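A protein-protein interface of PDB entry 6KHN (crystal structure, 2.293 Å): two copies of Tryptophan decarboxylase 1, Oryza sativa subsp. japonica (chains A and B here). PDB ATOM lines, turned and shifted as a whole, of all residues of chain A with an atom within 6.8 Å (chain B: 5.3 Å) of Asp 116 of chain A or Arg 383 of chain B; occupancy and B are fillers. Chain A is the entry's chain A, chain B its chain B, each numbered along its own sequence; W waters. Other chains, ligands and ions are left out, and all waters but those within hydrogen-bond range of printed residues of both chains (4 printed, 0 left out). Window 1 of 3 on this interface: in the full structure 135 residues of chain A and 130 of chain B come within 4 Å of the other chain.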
ATOM      1  N   ALA A 111      17.273 -26.867  10.808  1.00  0.00           N
ATOM      2  CA  ALA A 111      17.775 -27.640  11.942  1.00  0.00           C
ATOM      3  C   ALA A 111      16.903 -27.448  13.182  1.00  0.00           C
ATOM      4  O   ALA A 111      16.645 -28.412  13.912  1.00  0.00           O
ATOM      5  CB  ALA A 111      19.233 -27.272  12.245  1.00  0.00           C
ATOM      6  N   ALA A 112      16.461 -26.213  13.448  1.00  0.00           N
ATOM      7  CA  ALA A 112      15.602 -25.957  14.602  1.00  0.00           C
ATOM      8  C   ALA A 112      14.246 -26.630  14.437  1.00  0.00           C
ATOM      9  O   ALA A 112      13.713 -27.216  15.387  1.00  0.00           O
ATOM     10  CB  ALA A 112      15.414 -24.447  14.810  1.00  0.00           C
ATOM     11  N   ILE A 113      13.655 -26.529  13.247  1.00  0.00           N
ATOM     12  CA  ILE A 113      12.408 -27.243  13.002  1.00  0.00           C
ATOM     13  C   ILE A 113      12.606 -28.744  13.221  1.00  0.00           C
ATOM     14  O   ILE A 113      11.793 -29.395  13.886  1.00  0.00           O
ATOM     15  CB  ILE A 113      11.880 -26.913  11.597  1.00  0.00           C
ATOM     16  CG1 ILE A 113      11.677 -25.396  11.470  1.00  0.00           C
ATOM     17  CG2 ILE A 113      10.586 -27.616  11.340  1.00  0.00           C
ATOM     18  CD1 ILE A 113      11.277 -24.960  10.067  1.00  0.00           C
ATOM     19  N   ALA A 114      13.726 -29.298  12.735  1.00  0.00           N
ATOM     20  CA  ALA A 114      13.971 -30.731  12.914  1.00  0.00           C
ATOM     21  C   ALA A 114      14.139 -31.096  14.387  1.00  0.00           C
ATOM     22  O   ALA A 114      13.620 -32.129  14.839  1.00  0.00           O
ATOM     23  CB  ALA A 114      15.204 -31.162  12.119  1.00  0.00           C
ATOM     24  N   GLY A 115      14.860 -30.263  15.147  1.00  0.00           N
ATOM     25  CA  GLY A 115      15.024 -30.510  16.570  1.00  0.00           C
ATOM     26  C   GLY A 115      13.709 -30.493  17.329  1.00  0.00           C
ATOM     27  O   GLY A 115      13.443 -31.382  18.143  1.00  0.00           O
ATOM     28  N   ASP A 116      12.873 -29.474  17.083  1.00  0.00           N
ATOM     29  CA  ASP A 116      11.575 -29.411  17.756  1.00  0.00           C
ATOM     30  C   ASP A 116      10.682 -30.586  17.374  1.00  0.00           C
ATOM     31  O   ASP A 116       9.993 -31.153  18.229  1.00  0.00           O
ATOM     32  CB  ASP A 116      10.861 -28.093  17.449  1.00  0.00           C
ATOM     33  CG  ASP A 116      10.758 -27.199  18.671  1.00  0.00           C
ATOM     34  OD1 ASP A 116      11.064 -27.693  19.787  1.00  0.00           O
ATOM     35  OD2 ASP A 116      10.356 -26.016  18.532  1.00  0.00           O
ATOM     36  N   LEU A 117      10.676 -30.974  16.095  1.00  0.00           N
ATOM     37  CA  LEU A 117       9.910 -32.161  15.699  1.00  0.00           C
ATOM     38  C   LEU A 117      10.342 -33.384  16.502  1.00  0.00           C
ATOM     39  O   LEU A 117       9.507 -34.089  17.084  1.00  0.00           O
ATOM     40  CB  LEU A 117      10.050 -32.408  14.196  1.00  0.00           C
ATOM     41  CG  LEU A 117       9.618 -33.770  13.637  1.00  0.00           C
ATOM     42  CD1 LEU A 117       8.182 -34.092  14.002  1.00  0.00           C
ATOM     43  CD2 LEU A 117       9.809 -33.807  12.127  1.00  0.00           C
ATOM     44  N   ILE A 118      11.653 -33.625  16.586  1.00  0.00           N
ATOM     45  CA  ILE A 118      12.146 -34.776  17.337  1.00  0.00           C
ATOM     46  C   ILE A 118      11.759 -34.671  18.814  1.00  0.00           C
ATOM     47  O   ILE A 118      11.310 -35.654  19.422  1.00  0.00           O
ATOM     48  CB  ILE A 118      13.665 -34.923  17.135  1.00  0.00           C
ATOM     49  CG1 ILE A 118      13.940 -35.291  15.667  1.00  0.00           C
ATOM     50  CG2 ILE A 118      14.251 -35.977  18.098  1.00  0.00           C
ATOM     51  CD1 ILE A 118      15.406 -35.207  15.250  1.00  0.00           C
ATOM     52  N   ALA A 119      11.891 -33.474  19.406  1.00  0.00           N
ATOM     53  CA  ALA A 119      11.507 -33.301  20.802  1.00  0.00           C
ATOM     54  C   ALA A 119      10.014 -33.549  20.999  1.00  0.00           C
ATOM     55  O   ALA A 119       9.612 -34.207  21.967  1.00  0.00           O
ATOM     56  CB  ALA A 119      11.901 -31.902  21.297  1.00  0.00           C
ATOM     57  N   SER A 120       9.177 -33.034  20.091  1.00  0.00           N
ATOM     58  CA  SER A 120       7.739 -33.324  20.155  1.00  0.00           C
ATOM     59  C   SER A 120       7.446 -34.816  20.071  1.00  0.00           C
ATOM     60  O   SER A 120       6.470 -35.289  20.662  1.00  0.00           O
ATOM     61  CB  SER A 120       6.980 -32.621  19.024  1.00  0.00           C
ATOM     62  OG  SER A 120       6.991 -31.208  19.195  1.00  0.00           O
ATOM     63  N   ALA A 121       8.254 -35.572  19.331  1.00  0.00           N
ATOM     64  CA  ALA A 121       7.928 -36.985  19.176  1.00  0.00           C
ATOM     65  C   ALA A 121       8.419 -37.812  20.363  1.00  0.00           C
ATOM     66  O   ALA A 121       7.722 -38.725  20.817  1.00  0.00           O
ATOM     67  CB  ALA A 121       8.502 -37.513  17.866  1.00  0.00           C
ATOM     68  N   THR A 334      15.966 -20.083  15.714  1.00  0.00           N
ATOM     69  CA  THR A 334      15.420 -21.143  16.555  1.00  0.00           C
ATOM     70  C   THR A 334      13.944 -20.843  16.749  1.00  0.00           C
ATOM     71  O   THR A 334      13.605 -19.855  17.401  1.00  0.00           O
ATOM     72  CB  THR A 334      16.134 -21.193  17.911  1.00  0.00           C
ATOM     73  OG1 THR A 334      17.548 -21.340  17.718  1.00  0.00           O
ATOM     74  CG2 THR A 334      15.619 -22.341  18.757  1.00  0.00           C
ATOM     75  N   CYS A 335      13.069 -21.689  16.212  1.00  0.00           N
ATOM     76  CA  CYS A 335      11.635 -21.412  16.226  1.00  0.00           C
ATOM     77  C   CYS A 335      11.092 -21.304  17.652  1.00  0.00           C
ATOM     78  O   CYS A 335      11.625 -21.908  18.589  1.00  0.00           O
ATOM     79  CB  CYS A 335      10.897 -22.524  15.454  1.00  0.00           C
ATOM     80  SG  CYS A 335      11.101 -24.174  16.210  1.00  0.00           S
ATOM     81  N   LEU A 336      10.018 -20.519  17.815  1.00  0.00           N
ATOM     82  CA  LEU A 336       9.409 -20.335  19.136  1.00  0.00           C
ATOM     83  C   LEU A 336       9.003 -21.679  19.742  1.00  0.00           C
ATOM     84  O   LEU A 336       8.553 -22.578  19.027  1.00  0.00           O
ATOM     85  CB  LEU A 336       8.175 -19.433  19.036  1.00  0.00           C
ATOM     86  CG  LEU A 336       8.315 -17.919  18.840  1.00  0.00           C
ATOM     87  CD1 LEU A 336       8.633 -17.577  17.384  1.00  0.00           C
ATOM     88  CD2 LEU A 336       7.050 -17.179  19.323  1.00  0.00           C
ATOM     89  N   ASP A 337       9.125 -21.826  21.068  1.00  0.00           N
ATOM     90  CA  ASP A 337       9.612 -20.815  22.017  1.00  0.00           C
ATOM     91  C   ASP A 337      11.049 -21.130  22.458  1.00  0.00           C
ATOM     92  O   ASP A 337      11.419 -22.292  22.623  1.00  0.00           O
ATOM     93  CB  ASP A 337       8.715 -20.755  23.273  1.00  0.00           C
ATOM     94  CG  ASP A 337       7.220 -20.792  22.951  1.00  0.00           C
ATOM     95  OD1 ASP A 337       6.770 -20.033  22.064  1.00  0.00           O
ATOM     96  OD2 ASP A 337       6.489 -21.577  23.598  1.00  0.00           O
ATOM     97  N   ARG A 383       9.280 -29.007  28.125  1.00  0.00           N
ATOM     98  CA  ARG A 383       9.693 -29.680  26.910  1.00  0.00           C
ATOM     99  C   ARG A 383      11.215 -29.758  26.831  1.00  0.00           C
ATOM    100  O   ARG A 383      11.945 -29.048  27.532  1.00  0.00           O
ATOM    101  CB  ARG A 383       9.175 -28.932  25.687  1.00  0.00           C
ATOM    102  CG  ARG A 383       7.765 -29.221  25.338  1.00  0.00           C
ATOM    103  CD  ARG A 383       7.292 -28.259  24.257  1.00  0.00           C
ATOM    104  NE  ARG A 383       8.381 -27.916  23.363  1.00  0.00           N
ATOM    105  CZ  ARG A 383       8.681 -28.581  22.258  1.00  0.00           C
ATOM    106  NH1 ARG A 383       7.963 -29.625  21.876  1.00  0.00           N
ATOM    107  NH2 ARG A 383       9.712 -28.181  21.532  1.00  0.00           N
ATOM    108  N   PHE A 384      11.687 -30.609  25.916  1.00  0.00           N
ATOM    109  CA  PHE A 384      13.111 -30.723  25.591  1.00  0.00           C
ATOM    110  C   PHE A 384      13.505 -29.620  24.595  1.00  0.00           C
ATOM    111  O   PHE A 384      13.795 -29.853  23.422  1.00  0.00           O
ATOM    112  CB  PHE A 384      13.375 -32.126  25.056  1.00  0.00           C
ATOM    113  CG  PHE A 384      14.828 -32.470  24.859  1.00  0.00           C
ATOM    114  CD1 PHE A 384      15.838 -31.584  25.192  1.00  0.00           C
ATOM    115  CD2 PHE A 384      15.176 -33.711  24.325  1.00  0.00           C
ATOM    116  CE1 PHE A 384      17.161 -31.918  25.002  1.00  0.00           C
ATOM    117  CE2 PHE A 384      16.495 -34.056  24.129  1.00  0.00           C
ATOM    118  CZ  PHE A 384      17.498 -33.160  24.462  1.00  0.00           C
ATOM    119  N   ARG A 385      13.559 -28.381  25.099  1.00  0.00           N
ATOM    120  CA  ARG A 385      13.878 -27.261  24.217  1.00  0.00           C
ATOM    121  C   ARG A 385      15.369 -27.127  23.954  1.00  0.00           C
ATOM    122  O   ARG A 385      15.748 -26.453  22.988  1.00  0.00           O
ATOM    123  CB  ARG A 385      13.343 -25.943  24.780  1.00  0.00           C
ATOM    124  CG  ARG A 385      11.837 -25.856  24.780  1.00  0.00           C
ATOM    125  CD  ARG A 385      11.344 -24.425  24.683  1.00  0.00           C
ATOM    126  NE  ARG A 385      10.789 -23.950  25.942  1.00  0.00           N
ATOM    127  CZ  ARG A 385       9.509 -24.063  26.288  1.00  0.00           C
ATOM    128  NH1 ARG A 385       8.627 -24.621  25.457  1.00  0.00           N
ATOM    129  NH2 ARG A 385       9.107 -23.588  27.469  1.00  0.00           N
ATOM    130  N   LEU A 387      17.238 -29.325  22.680  1.00  0.00           N
ATOM    131  CA  LEU A 387      17.587 -30.065  21.471  1.00  0.00           C
ATOM    132  C   LEU A 387      17.659 -29.151  20.251  1.00  0.00           C
ATOM    133  O   LEU A 387      18.657 -29.157  19.524  1.00  0.00           O
ATOM    134  CB  LEU A 387      16.580 -31.193  21.240  1.00  0.00           C
ATOM    135  CG  LEU A 387      16.935 -32.165  20.110  1.00  0.00           C
ATOM    136  CD1 LEU A 387      18.249 -32.873  20.404  1.00  0.00           C
ATOM    137  CD2 LEU A 387      15.794 -33.176  19.858  1.00  0.00           C
ATOM    138  N   LYS A 388      16.604 -28.363  19.999  1.00  0.00           N
ATOM    139  CA  LYS A 388      16.595 -27.506  18.812  1.00  0.00           C
ATOM    140  C   LYS A 388      17.701 -26.458  18.875  1.00  0.00           C
ATOM    141  O   LYS A 388      18.341 -26.160  17.853  1.00  0.00           O
ATOM    142  CB  LYS A 388      15.225 -26.833  18.635  1.00  0.00           C
ATOM    143  CG  LYS A 388      14.851 -25.784  19.691  1.00  0.00           C
ATOM    144  CD  LYS A 388      13.488 -25.168  19.370  1.00  0.00           C
ATOM    145  CE  LYS A 388      12.860 -24.542  20.600  1.00  0.00           C
ATOM    146  NZ  LYS A 388      11.395 -24.259  20.404  1.00  0.00           N
ATOM    147  N   MET A 391      20.942 -28.165  18.131  1.00  0.00           N
ATOM    148  CA  MET A 391      21.011 -28.583  16.732  1.00  0.00           C
ATOM    149  C   MET A 391      21.368 -27.423  15.816  1.00  0.00           C
ATOM    150  O   MET A 391      22.110 -27.602  14.845  1.00  0.00           O
ATOM    151  CB  MET A 391      19.680 -29.204  16.300  1.00  0.00           C
ATOM    152  CG  MET A 391      19.515 -30.659  16.705  1.00  0.00           C
ATOM    153  SD  MET A 391      18.297 -31.545  15.695  1.00  0.00           S
ATOM    154  CE  MET A 391      18.573 -33.222  16.254  1.00  0.00           C
ATOM    155  N   ASP B 116       2.182 -29.782  15.563  1.00  0.00           N
ATOM    156  CA  ASP B 116       3.253 -28.978  16.149  1.00  0.00           C
ATOM    157  C   ASP B 116       4.400 -28.752  15.168  1.00  0.00           C
ATOM    158  O   ASP B 116       5.049 -27.699  15.214  1.00  0.00           O
ATOM    159  CB  ASP B 116       3.769 -29.611  17.441  1.00  0.00           C
ATOM    160  CG  ASP B 116       3.424 -28.769  18.678  1.00  0.00           C
ATOM    161  OD1 ASP B 116       2.842 -27.666  18.504  1.00  0.00           O
ATOM    162  OD2 ASP B 116       3.758 -29.189  19.813  1.00  0.00           O
ATOM    163  N   LEU B 117       4.656 -29.714  14.270  1.00  0.00           N
ATOM    164  CA  LEU B 117       5.658 -29.510  13.227  1.00  0.00           C
ATOM    165  C   LEU B 117       5.246 -28.394  12.271  1.00  0.00           C
ATOM    166  O   LEU B 117       6.077 -27.570  11.881  1.00  0.00           O
ATOM    167  CB  LEU B 117       5.882 -30.811  12.460  1.00  0.00           C
ATOM    168  CG  LEU B 117       6.544 -30.685  11.088  1.00  0.00           C
ATOM    169  CD1 LEU B 117       7.948 -30.133  11.226  1.00  0.00           C
ATOM    170  CD2 LEU B 117       6.565 -32.041  10.362  1.00  0.00           C
ATOM    171  N   ALA B 119       3.102 -25.906  12.931  1.00  0.00           N
ATOM    172  CA  ALA B 119       3.191 -24.655  13.689  1.00  0.00           C
ATOM    173  C   ALA B 119       4.633 -24.153  13.785  1.00  0.00           C
ATOM    174  O   ALA B 119       4.887 -22.953  13.629  1.00  0.00           O
ATOM    175  CB  ALA B 119       2.586 -24.843  15.075  1.00  0.00           C
ATOM    176  N   SER B 120       5.594 -25.058  14.014  1.00  0.00           N
ATOM    177  CA  SER B 120       6.994 -24.639  14.113  1.00  0.00           C
ATOM    178  C   SER B 120       7.482 -24.030  12.812  1.00  0.00           C
ATOM    179  O   SER B 120       8.343 -23.143  12.822  1.00  0.00           O
ATOM    180  CB  SER B 120       7.896 -25.827  14.471  1.00  0.00           C
ATOM    181  OG  SER B 120       7.663 -26.271  15.799  1.00  0.00           O
ATOM    182  N   THR B 124       4.516 -18.362  13.655  1.00  0.00           N
ATOM    183  CA  THR B 124       3.836 -17.093  13.902  1.00  0.00           C
ATOM    184  C   THR B 124       3.775 -16.798  15.400  1.00  0.00           C
ATOM    185  O   THR B 124       3.875 -17.691  16.248  1.00  0.00           O
ATOM    186  CB  THR B 124       2.411 -17.095  13.315  1.00  0.00           C
ATOM    187  OG1 THR B 124       1.630 -18.112  13.940  1.00  0.00           O
ATOM    188  CG2 THR B 124       2.424 -17.354  11.799  1.00  0.00           C
ATOM    189  N   GLU B 139      -7.256 -21.202  18.247  1.00  0.00           N
ATOM    190  CA  GLU B 139      -7.133 -21.475  19.676  1.00  0.00           C
ATOM    191  C   GLU B 139      -8.466 -21.284  20.390  1.00  0.00           C
ATOM    192  O   GLU B 139      -8.816 -22.072  21.274  1.00  0.00           O
ATOM    193  CB  GLU B 139      -6.039 -20.592  20.286  1.00  0.00           C
ATOM    194  CG  GLU B 139      -4.659 -20.884  19.679  1.00  0.00           C
ATOM    195  CD  GLU B 139      -3.501 -20.756  20.678  1.00  0.00           C
ATOM    196  OE1 GLU B 139      -2.354 -21.089  20.298  1.00  0.00           O
ATOM    197  OE2 GLU B 139      -3.736 -20.331  21.833  1.00  0.00           O
ATOM    198  N   GLY B 381       3.643 -13.168  23.949  1.00  0.00           N
ATOM    199  CA  GLY B 381       3.838 -13.770  22.654  1.00  0.00           C
ATOM    200  C   GLY B 381       4.559 -15.096  22.709  1.00  0.00           C
ATOM    201  O   GLY B 381       5.742 -15.167  23.067  1.00  0.00           O
ATOM    202  N   ARG B 382       3.847 -16.157  22.346  1.00  0.00           N
ATOM    203  CA  ARG B 382       4.399 -17.496  22.305  1.00  0.00           C
ATOM    204  C   ARG B 382       3.807 -18.208  21.091  1.00  0.00           C
ATOM    205  O   ARG B 382       3.014 -17.634  20.329  1.00  0.00           O
ATOM    206  CB  ARG B 382       4.136 -18.240  23.624  1.00  0.00           C
ATOM    207  CG  ARG B 382       2.765 -17.960  24.259  1.00  0.00           C
ATOM    208  CD  ARG B 382       1.641 -18.563  23.432  1.00  0.00           C
ATOM    209  NE  ARG B 382       0.324 -18.442  24.049  1.00  0.00           N
ATOM    210  CZ  ARG B 382      -0.772 -19.050  23.595  1.00  0.00           C
ATOM    211  NH1 ARG B 382      -0.715 -19.830  22.513  1.00  0.00           N
ATOM    212  NH2 ARG B 382      -1.929 -18.882  24.220  1.00  0.00           N
ATOM    213  N   ARG B 383       4.176 -19.474  20.915  1.00  0.00           N
ATOM    214  CA  ARG B 383       3.845 -20.158  19.673  1.00  0.00           C
ATOM    215  C   ARG B 383       2.362 -20.505  19.594  1.00  0.00           C
ATOM    216  O   ARG B 383       1.583 -20.356  20.543  1.00  0.00           O
ATOM    217  CB  ARG B 383       4.681 -21.425  19.501  1.00  0.00           C
ATOM    218  CG  ARG B 383       4.508 -22.465  20.574  1.00  0.00           C
ATOM    219  CD  ARG B 383       5.532 -23.556  20.371  1.00  0.00           C
ATOM    220  NE  ARG B 383       5.064 -24.521  19.386  1.00  0.00           N
ATOM    221  CZ  ARG B 383       5.827 -25.103  18.465  1.00  0.00           C
ATOM    222  NH1 ARG B 383       7.126 -24.832  18.386  1.00  0.00           N
ATOM    223  NH2 ARG B 383       5.284 -25.970  17.619  1.00  0.00           N
ATOM    224  N   PHE B 384       1.998 -20.984  18.418  1.00  0.00           N
ATOM    225  CA  PHE B 384       0.650 -21.352  18.004  1.00  0.00           C
ATOM    226  C   PHE B 384       0.346 -22.753  18.534  1.00  0.00           C
ATOM    227  O   PHE B 384       0.507 -23.759  17.836  1.00  0.00           O
ATOM    228  CB  PHE B 384       0.593 -21.267  16.479  1.00  0.00           C
ATOM    229  CG  PHE B 384      -0.728 -21.609  15.864  1.00  0.00           C
ATOM    230  CD1 PHE B 384      -1.882 -21.705  16.619  1.00  0.00           C
ATOM    231  CD2 PHE B 384      -0.810 -21.792  14.494  1.00  0.00           C
ATOM    232  CE1 PHE B 384      -3.083 -22.002  16.025  1.00  0.00           C
ATOM    233  CE2 PHE B 384      -2.009 -22.078  13.891  1.00  0.00           C
ATOM    234  CZ  PHE B 384      -3.150 -22.188  14.657  1.00  0.00           C
ATOM    235  N   ARG B 385      -0.130 -22.831  19.777  1.00  0.00           N
ATOM    236  CA  ARG B 385      -0.393 -24.140  20.375  1.00  0.00           C
ATOM    237  C   ARG B 385      -1.746 -24.744  19.992  1.00  0.00           C
ATOM    238  O   ARG B 385      -1.968 -25.932  20.251  1.00  0.00           O
ATOM    239  CB  ARG B 385      -0.270 -24.030  21.895  1.00  0.00           C
ATOM    240  CG  ARG B 385       0.966 -23.236  22.280  1.00  0.00           C
ATOM    241  CD  ARG B 385       1.507 -23.586  23.641  1.00  0.00           C
ATOM    242  NE  ARG B 385       1.005 -22.676  24.647  1.00  0.00           N
ATOM    243  CZ  ARG B 385       1.746 -21.956  25.494  1.00  0.00           C
ATOM    244  NH1 ARG B 385       3.077 -22.019  25.497  1.00  0.00           N
ATOM    245  NH2 ARG B 385       1.134 -21.159  26.353  1.00  0.00           N
HETATM  246  O   HOH W   1       6.089 -27.558  21.244  1.00  0.00           O
HETATM  247  O   HOH W   2       8.784 -28.861  14.724  1.00  0.00           O
HETATM  248  O   HOH W   3       7.183 -29.285  16.987  1.00  0.00           O
HETATM  249  O   HOH W   4       4.480 -23.680  24.203  1.00  0.00           O
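Water W4 bridges NH1 of Arg 385 of chain B (2.5 Å) and OD2 of Asp 337 of chain A (3.0 Å). Water W1 lies within hydrogen-bond range of NH1 of Arg 383 of chain A and OD2 of Asp 116 of chain B. Water W3 lies within hydrogen-bond range of OG of Ser 120 of chain A, O of Asp 116 of chain B and OG of Ser 120 of chain B. Water W2 lies within hydrogen-bond range of the side-chain hydroxyl of Ser 120 of chain B (3.0 Å), the backbone NH of Leu 117 of chain A (3.2 Å) and the backbone carbonyl oxygen of Ile 113 of chain A (3.2 Å).
Of chain B, only Ser 120 and Arg 383 come within 4 Å of Asp 116 of chain A. Of chain A, only Asp 116 (3.4 Å), Leu 336 (2.7 Å) and Asp 337 (2.9 Å) come within 4 Å of Arg 383 of chain B. Of the printed residues of chain A, Arg 385 of chain B touches Asp 337 (3.9 Å). Printed residues of chain B within 4 Å of Cys 335 of chain A: Ser 120 (3.7 Å). The nearest residue of chain A that does not touch Arg 383 of chain B is Cys 335 of chain A (4.6 Å). The nearest printed residue of chain B that does not touch Ile 113 of chain A is Ser 120 of chain B (4.2 Å).
OE1 of Glu 139 of chain B sits at hydrogen-bond distance from N of Arg 385 of chain B (2.9 Å). O of Asp 116 of chain A lies within hydrogen-bond range of OG of Ser 120 of chain A. The backbone carbonyl oxygen (O) of Cys 335 of chain A sits at hydrogen-bond distance from the side-chain amino group (NZ) of Lys 388 of chain A, at 3.0 Å. The backbone carbonyl oxygen (O) of Asp 116 of chain B lies within hydrogen-bond range of the side-chain hydroxyl (OG) of Ser 120 of chain B. OD2 of Asp 116 of chain A lies within salt-bridge range of NZ of Lys 388 of chain A (2.8 Å). The side-chain sulfur of Cys 335 of chain A is in hydrogen-bond range of the side-chain carboxylate of Asp 116 of chain A (3.1 Å).
OD1 of Asp 337 of chain A sits at hydrogen-bond distance from N of Arg 383 of chain B. The backbone carbonyl oxygen of Leu 336 of chain A lies within hydrogen-bond range of the guanidinium group of Arg 383 of chain B (2.7 Å). NH1 of Arg 383 of chain B lies within salt-bridge range of OD2 of Asp 116 of chain A. The side-chain carboxylate of Asp 337 of chain A is in salt-bridge range of the guanidinium group of Arg 385 of chain B (3.9 Å).
Of the 21 printed residues of chain A, 6 touch a printed residue of chain B. Printed residues of chain A that touch a printed residue of chain B: Ile 113, Asp 116, Ser 120, Cys 335, Leu 336 and Asp 337. Hydrophobic or aromatic side chains of chain A that line the printed part of chain B: Ile 113 and Leu 336. Of the 11 printed residues of chain B, 6 touch a printed residue of chain A. Hydrophobic or aromatic side chains of chain B that line the printed part of chain A: Leu 117. Among the printed residues, 10 pairs touch across the chains.
Among the printed residues, merely in contact across the chains: Ile 113 of chain A with Leu 117 of chain B (3.6 Å), Asp 116 of chain A with Ser 120 of chain B (3.8 Å), Ser 120 of chain A with Asp 116 of chain B (3.9 Å), Cys 335 of chain A with Ser 120 of chain B (3.7 Å), Leu 336 of chain A with Arg 382 of chain B (3.8 Å) and Asp 337 of chain A with Arg 382 of chain B (3.5 Å).
Asp 116 of chain A touches Ser 120 of chain B, and with the chains exchanged Ser 120 of chain A touches Asp 116 of chain B. Asp 116 of chain A touches Arg 383 of chain B, but with the chains exchanged Arg 383 of chain A does not touch Asp 116 of chain B (4.7 Å). Of the 10 pairs that touch across the chains among the printed residues, 2 have their exchanged pair printed and touching as well.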
